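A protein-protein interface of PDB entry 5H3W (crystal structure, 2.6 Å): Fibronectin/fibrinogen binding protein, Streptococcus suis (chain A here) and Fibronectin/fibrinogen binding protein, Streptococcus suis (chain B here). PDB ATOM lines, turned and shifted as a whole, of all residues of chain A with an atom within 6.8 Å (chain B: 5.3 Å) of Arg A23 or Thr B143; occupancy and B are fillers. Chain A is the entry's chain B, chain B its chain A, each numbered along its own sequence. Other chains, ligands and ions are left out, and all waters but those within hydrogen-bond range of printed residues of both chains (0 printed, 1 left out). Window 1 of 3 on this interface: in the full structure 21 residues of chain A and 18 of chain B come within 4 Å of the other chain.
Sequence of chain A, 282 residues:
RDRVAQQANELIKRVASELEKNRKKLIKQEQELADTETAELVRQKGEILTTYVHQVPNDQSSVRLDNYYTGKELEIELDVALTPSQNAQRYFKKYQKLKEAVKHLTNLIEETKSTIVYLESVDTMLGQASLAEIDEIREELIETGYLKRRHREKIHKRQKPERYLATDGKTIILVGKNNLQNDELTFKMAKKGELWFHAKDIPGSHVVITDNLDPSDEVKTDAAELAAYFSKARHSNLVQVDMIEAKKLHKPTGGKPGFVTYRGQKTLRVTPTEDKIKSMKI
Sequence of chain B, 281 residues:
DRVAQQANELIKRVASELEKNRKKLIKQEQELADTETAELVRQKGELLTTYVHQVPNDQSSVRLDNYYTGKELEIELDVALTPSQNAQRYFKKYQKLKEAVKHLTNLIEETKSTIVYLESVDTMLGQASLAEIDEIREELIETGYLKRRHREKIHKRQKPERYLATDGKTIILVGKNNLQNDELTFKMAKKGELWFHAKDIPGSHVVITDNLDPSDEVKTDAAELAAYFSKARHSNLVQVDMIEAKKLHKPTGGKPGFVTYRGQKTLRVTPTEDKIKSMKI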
ATOM      1  N   ALA A  16       4.429 -10.789  23.154  1.00  0.00           N
ATOM      2  CA  ALA A  16       5.711 -11.031  22.495  1.00  0.00           C
ATOM      3  C   ALA A  16       6.394 -12.300  23.031  1.00  0.00           C
ATOM      4  O   ALA A  16       7.023 -13.043  22.270  1.00  0.00           O
ATOM      5  CB  ALA A  16       6.622  -9.826  22.627  1.00  0.00           C
ATOM      6  N   GLU A  18       4.923 -14.936  24.086  1.00  0.00           N
ATOM      7  CA  GLU A  18       4.224 -16.033  23.445  1.00  0.00           C
ATOM      8  C   GLU A  18       4.720 -16.267  22.030  1.00  0.00           C
ATOM      9  O   GLU A  18       4.921 -17.409  21.637  1.00  0.00           O
ATOM     10  CB  GLU A  18       2.712 -15.791  23.461  1.00  0.00           C
ATOM     11  CG  GLU A  18       2.101 -16.009  24.827  1.00  0.00           C
ATOM     12  CD  GLU A  18       2.375 -17.416  25.325  1.00  0.00           C
ATOM     13  OE1 GLU A  18       2.389 -18.331  24.478  1.00  0.00           O
ATOM     14  OE2 GLU A  18       2.579 -17.615  26.545  1.00  0.00           O
ATOM     15  N   LEU A  19       4.914 -15.197  21.261  1.00  0.00           N
ATOM     16  CA  LEU A  19       5.430 -15.326  19.893  1.00  0.00           C
ATOM     17  C   LEU A  19       6.770 -16.017  19.921  1.00  0.00           C
ATOM     18  O   LEU A  19       7.010 -16.972  19.172  1.00  0.00           O
ATOM     19  CB  LEU A  19       5.562 -13.964  19.238  1.00  0.00           C
ATOM     20  CG  LEU A  19       4.283 -13.477  18.587  1.00  0.00           C
ATOM     21  CD1 LEU A  19       4.412 -12.033  18.160  1.00  0.00           C
ATOM     22  CD2 LEU A  19       3.978 -14.379  17.391  1.00  0.00           C
ATOM     23  N   GLU A  20       7.634 -15.518  20.806  1.00  0.00           N
ATOM     24  CA  GLU A  20       8.983 -16.055  20.992  1.00  0.00           C
ATOM     25  C   GLU A  20       8.946 -17.537  21.334  1.00  0.00           C
ATOM     26  O   GLU A  20       9.661 -18.324  20.722  1.00  0.00           O
ATOM     27  CB  GLU A  20       9.727 -15.297  22.101  1.00  0.00           C
ATOM     28  CG  GLU A  20      11.131 -15.820  22.369  1.00  0.00           C
ATOM     29  CD  GLU A  20      11.784 -15.205  23.608  1.00  0.00           C
ATOM     30  OE1 GLU A  20      11.055 -14.745  24.524  1.00  0.00           O
ATOM     31  OE2 GLU A  20      13.036 -15.211  23.680  1.00  0.00           O
ATOM     32  N   LYS A  21       8.089 -17.913  22.291  1.00  0.00           N
ATOM     33  CA  LYS A  21       7.978 -19.304  22.744  1.00  0.00           C
ATOM     34  C   LYS A  21       7.531 -20.207  21.591  1.00  0.00           C
ATOM     35  O   LYS A  21       8.122 -21.256  21.355  1.00  0.00           O
ATOM     36  CB  LYS A  21       7.013 -19.409  23.928  1.00  0.00           C
ATOM     37  CG  LYS A  21       6.909 -20.796  24.565  1.00  0.00           C
ATOM     38  CD  LYS A  21       5.533 -20.988  25.224  1.00  0.00           C
ATOM     39  CE  LYS A  21       5.582 -20.757  26.723  1.00  0.00           C
ATOM     40  NZ  LYS A  21       4.217 -20.567  27.307  1.00  0.00           N
ATOM     41  N   ASN A  22       6.527 -19.766  20.838  1.00  0.00           N
ATOM     42  CA  ASN A  22       6.021 -20.561  19.727  1.00  0.00           C
ATOM     43  C   ASN A  22       6.961 -20.648  18.530  1.00  0.00           C
ATOM     44  O   ASN A  22       6.956 -21.649  17.813  1.00  0.00           O
ATOM     45  CB  ASN A  22       4.654 -20.066  19.280  1.00  0.00           C
ATOM     46  CG  ASN A  22       3.549 -20.496  20.211  1.00  0.00           C
ATOM     47  OD1 ASN A  22       2.967 -21.574  20.045  1.00  0.00           O
ATOM     48  ND2 ASN A  22       3.257 -19.663  21.207  1.00  0.00           N
ATOM     49  N   ARG A  23       7.774 -19.616  18.309  1.00  0.00           N
ATOM     50  CA  ARG A  23       8.745 -19.688  17.230  1.00  0.00           C
ATOM     51  C   ARG A  23       9.840 -20.690  17.586  1.00  0.00           C
ATOM     52  O   ARG A  23      10.234 -21.480  16.747  1.00  0.00           O
ATOM     53  CB  ARG A  23       9.341 -18.301  16.929  1.00  0.00           C
ATOM     54  CG  ARG A  23       8.386 -17.416  16.157  1.00  0.00           C
ATOM     55  CD  ARG A  23       8.801 -15.957  16.136  1.00  0.00           C
ATOM     56  NE  ARG A  23       7.834 -15.187  15.348  1.00  0.00           N
ATOM     57  CZ  ARG A  23       7.569 -13.891  15.534  1.00  0.00           C
ATOM     58  NH1 ARG A  23       8.218 -13.200  16.489  1.00  0.00           N
ATOM     59  NH2 ARG A  23       6.663 -13.283  14.743  1.00  0.00           N
ATOM     60  N   LYS A  24      10.305 -20.673  18.837  1.00  0.00           N
ATOM     61  CA  LYS A  24      11.264 -21.657  19.344  1.00  0.00           C
ATOM     62  C   LYS A  24      10.654 -23.047  19.284  1.00  0.00           C
ATOM     63  O   LYS A  24      11.336 -24.047  19.027  1.00  0.00           O
ATOM     64  CB  LYS A  24      11.662 -21.341  20.799  1.00  0.00           C
ATOM     65  CG  LYS A  24      12.775 -20.324  20.924  1.00  0.00           C
ATOM     66  CD  LYS A  24      13.038 -19.893  22.366  1.00  0.00           C
ATOM     67  CE  LYS A  24      14.165 -18.843  22.422  1.00  0.00           C
ATOM     68  NZ  LYS A  24      14.299 -18.230  23.778  1.00  0.00           N
ATOM     69  N   LYS A  25       9.358 -23.110  19.556  1.00  0.00           N
ATOM     70  CA  LYS A  25       8.650 -24.371  19.496  1.00  0.00           C
ATOM     71  C   LYS A  25       8.572 -24.877  18.059  1.00  0.00           C
ATOM     72  O   LYS A  25       8.689 -26.080  17.813  1.00  0.00           O
ATOM     73  CB  LYS A  25       7.249 -24.204  20.076  1.00  0.00           C
ATOM     74  CG  LYS A  25       6.454 -25.472  20.115  1.00  0.00           C
ATOM     75  CD  LYS A  25       5.015 -25.096  20.328  1.00  0.00           C
ATOM     76  CE  LYS A  25       4.146 -26.242  20.749  1.00  0.00           C
ATOM     77  NZ  LYS A  25       3.004 -25.610  21.413  1.00  0.00           N
ATOM     78  N   LEU A  26       8.369 -23.962  17.116  1.00  0.00           N
ATOM     79  CA  LEU A  26       8.238 -24.347  15.715  1.00  0.00           C
ATOM     80  C   LEU A  26       9.497 -24.966  15.125  1.00  0.00           C
ATOM     81  O   LEU A  26       9.415 -25.974  14.411  1.00  0.00           O
ATOM     82  CB  LEU A  26       7.826 -23.169  14.854  1.00  0.00           C
ATOM     83  CG  LEU A  26       7.702 -23.584  13.396  1.00  0.00           C
ATOM     84  CD1 LEU A  26       6.606 -24.647  13.229  1.00  0.00           C
ATOM     85  CD2 LEU A  26       7.447 -22.343  12.571  1.00  0.00           C
ATOM     86  N   ILE A  27      10.648 -24.363  15.409  1.00  0.00           N
ATOM     87  CA  ILE A  27      11.928 -24.873  14.911  1.00  0.00           C
ATOM     88  C   ILE A  27      12.214 -26.235  15.568  1.00  0.00           C
ATOM     89  O   ILE A  27      12.792 -27.130  14.957  1.00  0.00           O
ATOM     90  CB  ILE A  27      13.078 -23.865  15.169  1.00  0.00           C
ATOM     91  CG1 ILE A  27      14.415 -24.369  14.628  1.00  0.00           C
ATOM     92  CG2 ILE A  27      13.201 -23.546  16.629  1.00  0.00           C
ATOM     93  CD1 ILE A  27      14.611 -24.115  13.172  1.00  0.00           C
ATOM     94  N   LYS A  28      11.789 -26.403  16.816  1.00  0.00           N
ATOM     95  CA  LYS A  28      11.992 -27.671  17.505  1.00  0.00           C
ATOM     96  C   LYS A  28      11.142 -28.751  16.827  1.00  0.00           C
ATOM     97  O   LYS A  28      11.612 -29.848  16.562  1.00  0.00           O
ATOM     98  CB  LYS A  28      11.641 -27.528  18.982  1.00  0.00           C
ATOM     99  CG  LYS A  28      12.814 -27.749  19.928  1.00  0.00           C
ATOM    100  CD  LYS A  28      13.986 -26.848  19.600  1.00  0.00           C
ATOM    101  CE  LYS A  28      15.228 -27.185  20.420  1.00  0.00           C
ATOM    102  NZ  LYS A  28      16.431 -26.427  19.913  1.00  0.00           N
ATOM    103  N   GLU A  30       9.964 -28.692  13.690  1.00  0.00           N
ATOM    104  CA  GLU A  30      10.472 -28.902  12.335  1.00  0.00           C
ATOM    105  C   GLU A  30      11.778 -29.706  12.362  1.00  0.00           C
ATOM    106  O   GLU A  30      12.027 -30.540  11.491  1.00  0.00           O
ATOM    107  CB  GLU A  30      10.680 -27.570  11.628  1.00  0.00           C
ATOM    108  CG  GLU A  30       9.398 -26.796  11.296  1.00  0.00           C
ATOM    109  CD  GLU A  30       9.688 -25.395  10.747  1.00  0.00           C
ATOM    110  OE1 GLU A  30      10.654 -24.754  11.244  1.00  0.00           O
ATOM    111  OE2 GLU A  30       8.963 -24.927   9.826  1.00  0.00           O
ATOM    112  N   THR A 112       1.061 -25.024  15.272  1.00  0.00           N
ATOM    113  CA  THR A 112       1.979 -24.050  15.817  1.00  0.00           C
ATOM    114  C   THR A 112       1.972 -22.805  14.920  1.00  0.00           C
ATOM    115  O   THR A 112       1.807 -21.686  15.413  1.00  0.00           O
ATOM    116  CB  THR A 112       3.390 -24.627  15.954  1.00  0.00           C
ATOM    117  OG1 THR A 112       3.339 -25.814  16.768  1.00  0.00           O
ATOM    118  CG2 THR A 112       4.324 -23.607  16.596  1.00  0.00           C
ATOM    119  N   ILE A 116       1.021 -18.890  15.668  1.00  0.00           N
ATOM    120  CA  ILE A 116       1.948 -17.798  15.425  1.00  0.00           C
ATOM    121  C   ILE A 116       1.247 -16.704  14.617  1.00  0.00           C
ATOM    122  O   ILE A 116       1.276 -15.527  14.992  1.00  0.00           O
ATOM    123  CB  ILE A 116       3.229 -18.293  14.744  1.00  0.00           C
ATOM    124  CG1 ILE A 116       4.028 -19.163  15.733  1.00  0.00           C
ATOM    125  CG2 ILE A 116       4.052 -17.106  14.253  1.00  0.00           C
ATOM    126  CD1 ILE A 116       5.105 -19.993  15.078  1.00  0.00           C
ATOM    127  N   GLU A 120       0.485 -13.000  15.944  1.00  0.00           N
ATOM    128  CA  GLU A 120       1.006 -11.885  15.141  1.00  0.00           C
ATOM    129  C   GLU A 120      -0.075 -10.853  14.878  1.00  0.00           C
ATOM    130  O   GLU A 120       0.165  -9.663  14.991  1.00  0.00           O
ATOM    131  CB  GLU A 120       1.671 -12.386  13.848  1.00  0.00           C
ATOM    132  CG  GLU A 120       3.084 -12.922  14.124  1.00  0.00           C
ATOM    133  CD  GLU A 120       3.728 -13.688  12.970  1.00  0.00           C
ATOM    134  OE1 GLU A 120       2.989 -14.251  12.112  1.00  0.00           O
ATOM    135  OE2 GLU A 120       4.992 -13.737  12.946  1.00  0.00           O
ATOM    136  N   LYS A 232       0.052  -4.327   9.317  1.00  0.00           N
ATOM    137  CA  LYS A 232       1.482  -4.375   9.588  1.00  0.00           C
ATOM    138  C   LYS A 232       2.263  -3.581   8.526  1.00  0.00           C
ATOM    139  O   LYS A 232       3.470  -3.349   8.678  1.00  0.00           O
ATOM    140  CB  LYS A 232       1.966  -5.835   9.637  1.00  0.00           C
ATOM    141  CG  LYS A 232       3.256  -6.064  10.427  1.00  0.00           C
ATOM    142  CD  LYS A 232       3.764  -7.477  10.267  1.00  0.00           C
ATOM    143  CE  LYS A 232       4.461  -7.957  11.523  1.00  0.00           C
ATOM    144  NZ  LYS A 232       5.391  -6.915  12.027  1.00  0.00           N
ATOM    145  N   TYR B 117      18.025  -3.031  16.810  1.00  0.00           N
ATOM    146  CA  TYR B 117      18.210  -4.442  16.511  1.00  0.00           C
ATOM    147  C   TYR B 117      18.379  -4.664  14.999  1.00  0.00           C
ATOM    148  O   TYR B 117      19.348  -5.287  14.555  1.00  0.00           O
ATOM    149  CB  TYR B 117      17.058  -5.289  17.060  1.00  0.00           C
ATOM    150  CG  TYR B 117      17.051  -6.648  16.437  1.00  0.00           C
ATOM    151  CD1 TYR B 117      17.972  -7.611  16.842  1.00  0.00           C
ATOM    152  CD2 TYR B 117      16.182  -6.950  15.391  1.00  0.00           C
ATOM    153  CE1 TYR B 117      18.004  -8.859  16.252  1.00  0.00           C
ATOM    154  CE2 TYR B 117      16.210  -8.200  14.784  1.00  0.00           C
ATOM    155  CZ  TYR B 117      17.123  -9.148  15.230  1.00  0.00           C
ATOM    156  OH  TYR B 117      17.175 -10.385  14.637  1.00  0.00           O
ATOM    157  N   GLU B 139      18.362 -16.516  12.375  1.00  0.00           N
ATOM    158  CA  GLU B 139      18.043 -15.498  13.379  1.00  0.00           C
ATOM    159  C   GLU B 139      16.782 -14.710  13.013  1.00  0.00           C
ATOM    160  O   GLU B 139      16.002 -14.332  13.897  1.00  0.00           O
ATOM    161  CB  GLU B 139      19.223 -14.543  13.566  1.00  0.00           C
ATOM    162  CG  GLU B 139      19.014 -13.502  14.667  1.00  0.00           C
ATOM    163  CD  GLU B 139      19.920 -12.288  14.514  1.00  0.00           C
ATOM    164  OE1 GLU B 139      21.144 -12.457  14.305  1.00  0.00           O
ATOM    165  OE2 GLU B 139      19.398 -11.156  14.574  1.00  0.00           O
ATOM    166  N   LEU B 140      16.596 -14.436  11.715  1.00  0.00           N
ATOM    167  CA  LEU B 140      15.458 -13.631  11.249  1.00  0.00           C
ATOM    168  C   LEU B 140      14.141 -14.430  11.257  1.00  0.00           C
ATOM    169  O   LEU B 140      13.036 -13.870  11.433  1.00  0.00           O
ATOM    170  CB  LEU B 140      15.758 -13.061   9.860  1.00  0.00           C
ATOM    171  CG  LEU B 140      16.887 -12.013   9.844  1.00  0.00           C
ATOM    172  CD1 LEU B 140      17.350 -11.679   8.418  1.00  0.00           C
ATOM    173  CD2 LEU B 140      16.466 -10.732  10.585  1.00  0.00           C
ATOM    174  N   ILE B 141      14.276 -15.741  11.062  1.00  0.00           N
ATOM    175  CA  ILE B 141      13.185 -16.662  11.265  1.00  0.00           C
ATOM    176  C   ILE B 141      12.763 -16.660  12.747  1.00  0.00           C
ATOM    177  O   ILE B 141      11.567 -16.690  13.073  1.00  0.00           O
ATOM    178  CB  ILE B 141      13.593 -18.063  10.841  1.00  0.00           C
ATOM    179  CG1 ILE B 141      13.649 -18.139   9.312  1.00  0.00           C
ATOM    180  CG2 ILE B 141      12.636 -19.094  11.399  1.00  0.00           C
ATOM    181  CD1 ILE B 141      14.110 -19.495   8.796  1.00  0.00           C
ATOM    182  N   GLU B 142      13.748 -16.609  13.636  1.00  0.00           N
ATOM    183  CA  GLU B 142      13.488 -16.638  15.071  1.00  0.00           C
ATOM    184  C   GLU B 142      12.909 -15.332  15.640  1.00  0.00           C
ATOM    185  O   GLU B 142      12.164 -15.356  16.619  1.00  0.00           O
ATOM    186  CB  GLU B 142      14.766 -17.027  15.820  1.00  0.00           C
ATOM    187  CG  GLU B 142      14.604 -16.985  17.319  1.00  0.00           C
ATOM    188  CD  GLU B 142      15.688 -17.761  18.031  1.00  0.00           C
ATOM    189  OE1 GLU B 142      15.986 -17.432  19.201  1.00  0.00           O
ATOM    190  OE2 GLU B 142      16.214 -18.727  17.431  1.00  0.00           O
ATOM    191  N   THR B 143      13.268 -14.197  15.050  1.00  0.00           N
ATOM    192  CA  THR B 143      12.792 -12.896  15.527  1.00  0.00           C
ATOM    193  C   THR B 143      11.553 -12.475  14.750  1.00  0.00           C
ATOM    194  O   THR B 143      10.989 -11.412  14.972  1.00  0.00           O
ATOM    195  CB  THR B 143      13.886 -11.795  15.424  1.00  0.00           C
ATOM    196  OG1 THR B 143      14.483 -11.814  14.111  1.00  0.00           O
ATOM    197  CG2 THR B 143      14.971 -12.035  16.463  1.00  0.00           C
ATOM    198  N   GLY B 144      11.152 -13.322  13.815  1.00  0.00           N
ATOM    199  CA  GLY B 144       9.857 -13.189  13.176  1.00  0.00           C
ATOM    200  C   GLY B 144       9.812 -12.519  11.825  1.00  0.00           C
ATOM    201  O   GLY B 144       8.714 -12.343  11.291  1.00  0.00           O
ATOM    202  N   TYR B 145      10.973 -12.204  11.239  1.00  0.00           N
ATOM    203  CA  TYR B 145      10.984 -11.479   9.953  1.00  0.00           C
ATOM    204  C   TYR B 145      10.969 -12.396   8.740  1.00  0.00           C
ATOM    205  O   TYR B 145      10.721 -11.950   7.631  1.00  0.00           O
ATOM    206  CB  TYR B 145      12.178 -10.514   9.852  1.00  0.00           C
ATOM    207  CG  TYR B 145      12.102  -9.381  10.834  1.00  0.00           C
ATOM    208  CD1 TYR B 145      11.433  -8.202  10.517  1.00  0.00           C
ATOM    209  CD2 TYR B 145      12.686  -9.495  12.083  1.00  0.00           C
ATOM    210  CE1 TYR B 145      11.338  -7.168  11.430  1.00  0.00           C
ATOM    211  CE2 TYR B 145      12.592  -8.480  13.007  1.00  0.00           C
ATOM    212  CZ  TYR B 145      11.927  -7.317  12.669  1.00  0.00           C
ATOM    213  OH  TYR B 145      11.857  -6.306  13.596  1.00  0.00           O
ATOM    214  N   PRO B 256      17.925 -10.593  20.226  1.00  0.00           N
ATOM    215  CA  PRO B 256      19.219 -11.274  20.119  1.00  0.00           C
ATOM    216  C   PRO B 256      20.352 -10.262  19.966  1.00  0.00           C
ATOM    217  O   PRO B 256      20.203  -9.315  19.229  1.00  0.00           O
ATOM    218  CB  PRO B 256      19.075 -12.082  18.832  1.00  0.00           C
ATOM    219  CG  PRO B 256      17.621 -12.322  18.686  1.00  0.00           C
ATOM    220  CD  PRO B 256      16.957 -11.100  19.234  1.00  0.00           C
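NH2 of Arg A23 lies within salt-bridge range of OE2 of Glu A120, at 2.5 Å. The side-chain carboxylate of Glu A20 lies within salt-bridge range of the side-chain amino group of Lys A24 (3.3 Å). The backbone carbonyl oxygen (O) of Glu B139 sits at hydrogen-bond distance from the side-chain hydroxyl (OG1) of Thr B143 (2.9 Å). OG1 of Thr B143 lies within hydrogen-bond range of OH of Tyr B117.
Arg A23 touches Glu B142. NH1 of Arg A23 touches O of Thr B143 (3.6 Å). CZ of Arg A23 touches CA of Gly B144, at 3.4 Å. Glu B142 touches Lys A24.
Of the printed residues of chain B, Arg A23 touches Glu B142, Thr B143 and Gly B144. Ile A27 touches none of the printed residues of chain B. Leu B140 touches none of the printed residues of chain A. Of the printed residues of chain A, Glu B142 touches Arg A23 and Lys A24. Thr B143 touches just one residue of chain A: Arg A23 (3.6 Å). Printed residues of chain A within 4 Å of Gly B144: Arg A23 (3.4 Å). The nearest residue of chain A that does not touch Thr B143 is Glu A120 (6.7 Å).
Of the 9 printed residues of chain B, 3 touch a printed residue of chain A. Of the 17 printed residues of chain A, 2 touch a printed residue of chain B. Among the printed residues, no Asp or Glu carboxylate lies within 4 Å of a Lys or Arg side-chain nitrogen of the other chain.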
